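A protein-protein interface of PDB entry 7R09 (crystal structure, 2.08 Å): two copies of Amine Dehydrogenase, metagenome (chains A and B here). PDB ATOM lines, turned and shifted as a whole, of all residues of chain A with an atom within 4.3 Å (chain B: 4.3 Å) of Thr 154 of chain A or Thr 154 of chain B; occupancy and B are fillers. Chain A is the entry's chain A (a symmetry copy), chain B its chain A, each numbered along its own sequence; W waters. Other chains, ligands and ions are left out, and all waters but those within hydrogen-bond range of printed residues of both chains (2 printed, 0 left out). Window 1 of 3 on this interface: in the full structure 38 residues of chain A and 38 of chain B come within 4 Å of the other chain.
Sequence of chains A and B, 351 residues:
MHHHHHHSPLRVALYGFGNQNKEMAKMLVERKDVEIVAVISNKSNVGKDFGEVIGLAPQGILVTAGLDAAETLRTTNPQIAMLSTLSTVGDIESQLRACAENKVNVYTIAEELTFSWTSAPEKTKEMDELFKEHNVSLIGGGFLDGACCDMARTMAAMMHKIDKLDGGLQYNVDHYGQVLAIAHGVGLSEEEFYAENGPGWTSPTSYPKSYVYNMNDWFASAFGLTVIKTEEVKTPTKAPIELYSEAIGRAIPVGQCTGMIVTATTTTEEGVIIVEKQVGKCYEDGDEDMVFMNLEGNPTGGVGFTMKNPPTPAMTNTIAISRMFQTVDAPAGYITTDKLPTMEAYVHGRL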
ATOM      1  N   ASP A 150      14.063  22.848  -3.607  1.00  0.00           N
ATOM      2  CA  ASP A 150      13.779  24.295  -3.808  1.00  0.00           C
ATOM      3  C   ASP A 150      13.372  24.920  -2.471  1.00  0.00           C
ATOM      4  O   ASP A 150      13.854  26.014  -2.185  1.00  0.00           O
ATOM      5  CB  ASP A 150      12.760  24.534  -4.933  1.00  0.00           C
ATOM      6  CG  ASP A 150      12.907  25.881  -5.619  1.00  0.00           C
ATOM      7  OD1 ASP A 150      13.949  26.547  -5.406  1.00  0.00           O
ATOM      8  OD2 ASP A 150      11.988  26.258  -6.371  1.00  0.00           O
ATOM      9  N   MET A 151      12.555  24.239  -1.664  1.00  0.00           N
ATOM     10  CA  MET A 151      12.233  24.665  -0.274  1.00  0.00           C
ATOM     11  C   MET A 151      13.541  24.827   0.515  1.00  0.00           C
ATOM     12  O   MET A 151      13.722  25.879   1.183  1.00  0.00           O
ATOM     13  CB  MET A 151      11.356  23.632   0.446  1.00  0.00           C
ATOM     14  CG  MET A 151       9.900  23.628  -0.013  1.00  0.00           C
ATOM     15  SD  MET A 151       8.995  25.071   0.573  1.00  0.00           S
ATOM     16  CE  MET A 151       8.814  24.699   2.312  1.00  0.00           C
ATOM     17  N   ALA A 152      14.412  23.813   0.464  1.00  0.00           N
ATOM     18  CA  ALA A 152      15.752  23.836   1.109  1.00  0.00           C
ATOM     19  C   ALA A 152      16.531  25.048   0.613  1.00  0.00           C
ATOM     20  O   ALA A 152      17.246  25.632   1.416  1.00  0.00           O
ATOM     21  CB  ALA A 152      16.509  22.567   0.825  1.00  0.00           C
ATOM     22  N   ARG A 153      16.422  25.376  -0.678  1.00  0.00           N
ATOM     23  CA  ARG A 153      17.252  26.436  -1.303  1.00  0.00           C
ATOM     24  C   ARG A 153      16.831  27.785  -0.723  1.00  0.00           C
ATOM     25  O   ARG A 153      17.722  28.609  -0.461  1.00  0.00           O
ATOM     26  CB  ARG A 153      17.117  26.425  -2.828  1.00  0.00           C
ATOM     27  CG  ARG A 153      17.791  27.614  -3.500  1.00  0.00           C
ATOM     28  CD  ARG A 153      17.983  27.444  -4.992  1.00  0.00           C
ATOM     29  NE  ARG A 153      16.725  27.405  -5.720  1.00  0.00           N
ATOM     30  CZ  ARG A 153      16.582  27.673  -7.021  1.00  0.00           C
ATOM     31  NH1 ARG A 153      17.623  27.996  -7.769  1.00  0.00           N
ATOM     32  NH2 ARG A 153      15.382  27.645  -7.572  1.00  0.00           N
ATOM     33  N   THR A 154      15.519  28.007  -0.591  1.00  0.00           N
ATOM     34  CA  THR A 154      14.942  29.227   0.021  1.00  0.00           C
ATOM     35  C   THR A 154      15.479  29.350   1.443  1.00  0.00           C
ATOM     36  O   THR A 154      16.004  30.417   1.778  1.00  0.00           O
ATOM     37  CB  THR A 154      13.409  29.205   0.035  1.00  0.00           C
ATOM     38  OG1 THR A 154      12.934  29.233  -1.307  1.00  0.00           O
ATOM     39  CG2 THR A 154      12.826  30.366   0.805  1.00  0.00           C
ATOM     40  N   MET A 155      15.355  28.292   2.235  1.00  0.00           N
ATOM     41  CA  MET A 155      15.739  28.293   3.663  1.00  0.00           C
ATOM     42  C   MET A 155      17.261  28.459   3.801  1.00  0.00           C
ATOM     43  O   MET A 155      17.691  29.144   4.759  1.00  0.00           O
ATOM     44  CB  MET A 155      15.320  26.993   4.350  1.00  0.00           C
ATOM     45  CG  MET A 155      15.636  26.998   5.828  1.00  0.00           C
ATOM     46  SD  MET A 155      15.112  25.497   6.695  1.00  0.00           S
ATOM     47  CE  MET A 155      16.118  24.257   5.890  1.00  0.00           C
ATOM     48  N   ALA A 156      18.039  27.855   2.901  1.00  0.00           N
ATOM     49  CA  ALA A 156      19.526  27.928   2.917  1.00  0.00           C
ATOM     50  C   ALA A 156      19.987  29.376   2.725  1.00  0.00           C
ATOM     51  O   ALA A 156      21.099  29.692   3.151  1.00  0.00           O
ATOM     52  CB  ALA A 156      20.119  27.038   1.866  1.00  0.00           C
ATOM     53  N   ALA A 157      19.168  30.234   2.110  1.00  0.00           N
ATOM     54  CA  ALA A 157      19.562  31.625   1.814  1.00  0.00           C
ATOM     55  C   ALA A 157      19.841  32.308   3.147  1.00  0.00           C
ATOM     56  O   ALA A 157      20.589  33.280   3.162  1.00  0.00           O
ATOM     57  CB  ALA A 157      18.486  32.316   1.004  1.00  0.00           C
ATOM     58  N   THR A 342      13.073  30.279  -8.122  1.00  0.00           N
ATOM     59  CA  THR A 342      12.099  29.524  -7.286  1.00  0.00           C
ATOM     60  C   THR A 342      10.892  29.152  -8.152  1.00  0.00           C
ATOM     61  O   THR A 342      10.572  29.933  -9.046  1.00  0.00           O
ATOM     62  CB  THR A 342      11.741  30.374  -6.057  1.00  0.00           C
ATOM     63  OG1 THR A 342      12.981  30.769  -5.465  1.00  0.00           O
ATOM     64  CG2 THR A 342      10.907  29.668  -5.017  1.00  0.00           C
ATOM     65  N   MET A 343      10.237  28.024  -7.879  1.00  0.00           N
ATOM     66  CA  MET A 343       8.927  27.646  -8.485  1.00  0.00           C
ATOM     67  C   MET A 343       8.080  28.915  -8.644  1.00  0.00           C
ATOM     68  O   MET A 343       8.043  29.692  -7.694  1.00  0.00           O
ATOM     69  CB  MET A 343       8.146  26.670  -7.598  1.00  0.00           C
ATOM     70  CG  MET A 343       8.795  25.325  -7.452  1.00  0.00           C
ATOM     71  SD  MET A 343       8.002  24.308  -6.191  1.00  0.00           S
ATOM     72  CE  MET A 343       8.489  25.127  -4.678  1.00  0.00           C
ATOM     73  N   ASP B 150       8.615  34.679   2.976  1.00  0.00           N
ATOM     74  CA  ASP B 150       9.332  34.223   1.754  1.00  0.00           C
ATOM     75  C   ASP B 150       9.343  32.693   1.718  1.00  0.00           C
ATOM     76  O   ASP B 150       9.102  32.148   0.642  1.00  0.00           O
ATOM     77  CB  ASP B 150      10.729  34.851   1.635  1.00  0.00           C
ATOM     78  CG  ASP B 150      11.226  34.977   0.205  1.00  0.00           C
ATOM     79  OD1 ASP B 150      10.403  34.813  -0.727  1.00  0.00           O
ATOM     80  OD2 ASP B 150      12.428  35.250   0.026  1.00  0.00           O
ATOM     81  N   MET B 151       9.570  32.023   2.850  1.00  0.00           N
ATOM     82  CA  MET B 151       9.433  30.545   2.970  1.00  0.00           C
ATOM     83  C   MET B 151       8.017  30.137   2.534  1.00  0.00           C
ATOM     84  O   MET B 151       7.883  29.191   1.714  1.00  0.00           O
ATOM     85  CB  MET B 151       9.653  30.072   4.413  1.00  0.00           C
ATOM     86  CG  MET B 151      11.114  30.087   4.855  1.00  0.00           C
ATOM     87  SD  MET B 151      12.074  28.772   4.087  1.00  0.00           S
ATOM     88  CE  MET B 151      11.463  27.331   4.951  1.00  0.00           C
ATOM     89  N   ALA B 152       6.996  30.807   3.079  1.00  0.00           N
ATOM     90  CA  ALA B 152       5.571  30.588   2.716  1.00  0.00           C
ATOM     91  C   ALA B 152       5.400  30.769   1.212  1.00  0.00           C
ATOM     92  O   ALA B 152       4.616  30.028   0.636  1.00  0.00           O
ATOM     93  CB  ALA B 152       4.671  31.531   3.468  1.00  0.00           C
ATOM     94  N   ARG B 153       6.082  31.753   0.619  1.00  0.00           N
ATOM     95  CA  ARG B 153       5.875  32.120  -0.805  1.00  0.00           C
ATOM     96  C   ARG B 153       6.386  30.976  -1.678  1.00  0.00           C
ATOM     97  O   ARG B 153       5.719  30.666  -2.679  1.00  0.00           O
ATOM     98  CB  ARG B 153       6.579  33.434  -1.151  1.00  0.00           C
ATOM     99  CG  ARG B 153       6.563  33.751  -2.641  1.00  0.00           C
ATOM    100  CD  ARG B 153       6.923  35.186  -2.964  1.00  0.00           C
ATOM    101  NE  ARG B 153       8.303  35.505  -2.639  1.00  0.00           N
ATOM    102  CZ  ARG B 153       9.003  36.513  -3.169  1.00  0.00           C
ATOM    103  NH1 ARG B 153       8.460  37.328  -4.056  1.00  0.00           N
ATOM    104  NH2 ARG B 153      10.267  36.687  -2.829  1.00  0.00           N
ATOM    105  N   THR B 154       7.552  30.421  -1.333  1.00  0.00           N
ATOM    106  CA  THR B 154       8.153  29.256  -2.024  1.00  0.00           C
ATOM    107  C   THR B 154       7.164  28.097  -1.959  1.00  0.00           C
ATOM    108  O   THR B 154       6.858  27.532  -3.013  1.00  0.00           O
ATOM    109  CB  THR B 154       9.495  28.840  -1.409  1.00  0.00           C
ATOM    110  OG1 THR B 154      10.440  29.887  -1.610  1.00  0.00           O
ATOM    111  CG2 THR B 154      10.025  27.557  -2.004  1.00  0.00           C
ATOM    112  N   MET B 155       6.684  27.772  -0.765  1.00  0.00           N
ATOM    113  CA  MET B 155       5.795  26.613  -0.531  1.00  0.00           C
ATOM    114  C   MET B 155       4.443  26.837  -1.227  1.00  0.00           C
ATOM    115  O   MET B 155       3.877  25.843  -1.741  1.00  0.00           O
ATOM    116  CB  MET B 155       5.551  26.395   0.962  1.00  0.00           C
ATOM    117  CG  MET B 155       4.703  25.173   1.231  1.00  0.00           C
ATOM    118  SD  MET B 155       4.428  24.844   2.991  1.00  0.00           S
ATOM    119  CE  MET B 155       3.518  26.303   3.483  1.00  0.00           C
ATOM    120  N   ALA B 156       3.940  28.073  -1.235  1.00  0.00           N
ATOM    121  CA  ALA B 156       2.641  28.430  -1.869  1.00  0.00           C
ATOM    122  C   ALA B 156       2.697  28.166  -3.376  1.00  0.00           C
ATOM    123  O   ALA B 156       1.636  27.967  -3.971  1.00  0.00           O
ATOM    124  CB  ALA B 156       2.284  29.860  -1.593  1.00  0.00           C
ATOM    125  N   ALA B 157       3.889  28.159  -3.983  1.00  0.00           N
ATOM    126  CA  ALA B 157       4.028  27.991  -5.442  1.00  0.00           C
ATOM    127  C   ALA B 157       3.450  26.625  -5.797  1.00  0.00           C
ATOM    128  O   ALA B 157       3.046  26.439  -6.938  1.00  0.00           O
ATOM    129  CB  ALA B 157       5.475  28.150  -5.854  1.00  0.00           C
ATOM    130  N   THR B 342      13.226  35.539  -4.412  1.00  0.00           N
ATOM    131  CA  THR B 342      13.560  34.830  -3.146  1.00  0.00           C
ATOM    132  C   THR B 342      14.860  35.414  -2.584  1.00  0.00           C
ATOM    133  O   THR B 342      15.696  35.817  -3.389  1.00  0.00           O
ATOM    134  CB  THR B 342      13.630  33.321  -3.430  1.00  0.00           C
ATOM    135  OG1 THR B 342      12.414  32.980  -4.098  1.00  0.00           O
ATOM    136  CG2 THR B 342      13.776  32.450  -2.206  1.00  0.00           C
ATOM    137  N   MET B 343      15.029  35.431  -1.262  1.00  0.00           N
ATOM    138  CA  MET B 343      16.318  35.760  -0.586  1.00  0.00           C
ATOM    139  C   MET B 343      17.468  35.185  -1.422  1.00  0.00           C
ATOM    140  O   MET B 343      17.343  34.036  -1.839  1.00  0.00           O
ATOM    141  CB  MET B 343      16.403  35.142   0.815  1.00  0.00           C
ATOM    142  CG  MET B 343      15.413  35.706   1.792  1.00  0.00           C
ATOM    143  SD  MET B 343      15.354  34.771   3.333  1.00  0.00           S
ATOM    144  CE  MET B 343      14.560  33.250   2.826  1.00  0.00           C
HETATM  145  O   HOH W   1      17.302  31.108  -2.129  1.00  0.00           O
HETATM  146  O   HOH W   2       7.404  31.064  -5.170  1.00  0.00           O
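The side-chain sulfur (SD) of Met 151 of chain A sits close to the backbone NH (N) of Met 155 of chain B, at 3.8 Å. N of Met 155 of chain A sits close to SD of Met 151 of chain B, at 3.8 Å. The side-chain hydroxyl (OG1) of Thr 154 of chain B sits at hydrogen-bond distance from the side-chain hydroxyl (OG1) of Thr 154 of chain A (2.6 Å). OG1 of Thr 342 of chain A is in hydrogen-bond range of OG1 of Thr 342 of chain B, at 2.7 Å.
The side-chain carboxylate of Asp 150 of chain B lies within hydrogen-bond range of the backbone NH of Met 343 of chain B. The backbone carbonyl oxygen of Asp 150 of chain A lies within hydrogen-bond range of the side-chain hydroxyl of Thr 154 of chain A, 3.5 Å away. The side-chain hydroxyl (OG1) of Thr 154 of chain B is in hydrogen-bond range of the backbone carbonyl oxygen (O) of Asp 150 of chain B (3.5 Å). OD2 of Asp 150 of chain A sits at hydrogen-bond distance from N of Met 343 of chain A (2.9 Å).
Thr 154 of chain B touches Met 151 of chain A. Met 151 of chain B touches Thr 154 of chain A. OG1 of Thr 154 of chain A touches CG2 of Thr 342 of chain B, at 3.4 Å. Thr 154 of chain A touches Met 343 of chain B (O to CE, 3.3 Å). Met 343 of chain B touches Ala 157 of chain A (O to CB, 3.5 Å). OG1 of Thr 154 of chain B touches CG2 of Thr 342 of chain A, at 3.4 Å. Met 343 of chain A touches Thr 154 of chain B (CE to O, 3.3 Å). CB of Ala 157 of chain B touches O of Met 343 of chain A (3.5 Å).
Printed residues of chain B within 4 Å of Met 155 of chain A: Met 151 (3.7 Å). Ala 156 of chain A touches none of the printed residues of chain B. Printed residues of chain B within 4 Å of Thr 342 of chain A: Thr 154 (3.4 Å) and Thr 342 (2.7 Å). Of the printed residues of chain A, Met 151 of chain B touches Thr 154 (3.7 Å) and Met 155 (3.7 Å). Thr 154 of chain B touches just these residues of chain A: Met 151, Thr 154, Thr 342 and Met 343. Of the printed residues of chain A, Ala 157 of chain B touches Met 343 (3.5 Å). Of the printed residues of chain A, Thr 342 of chain B touches Thr 154 (3.4 Å) and Thr 342 (2.7 Å). The nearest residue of chain A that does not touch Thr 154 of chain B is Asp 150 of chain A (4.1 Å). The nearest printed residue of chain B that does not touch Ala 157 of chain A is Thr 342 of chain B (5.7 Å).
Of the 10 printed residues of chain B, 6 touch a printed residue of chain A. Hydrophobic or aromatic side chains of chain B within 4 Å of the printed part of chain A: Met 151, Met 155, Ala 157 and Met 343. Hydrophobic or aromatic side chains of chain A that line the printed part of chain B: Met 151, Met 155, Ala 157 and Met 343. Along chain A the printed residues that touch a printed residue of chain B span positions 151 to 343.
Met 151 of chain A touches Met 155 of chain B, and with the chains exchanged Met 155 of chain A touches Met 151 of chain B. Thr 154 of chain A touches Thr 342 of chain B, and with the chains exchanged Thr 342 of chain A touches Thr 154 of chain B. Ala 157 of chain A touches Met 343 of chain B, and with the chains exchanged Met 343 of chain A touches Ala 157 of chain B. Thr 342 of chain A touches its own counterpart, Thr 342 of chain B. Of the 12 pairs that touch across the chains among the printed residues, 12 have their exchanged pair printed and touching as well.
Water W1 bridges O of Met 343 of chain B and O of Arg 153 of chain A. Water W2 lies within hydrogen-bond range of O of Met 343 of chain A and O of Arg 153 of chain B.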
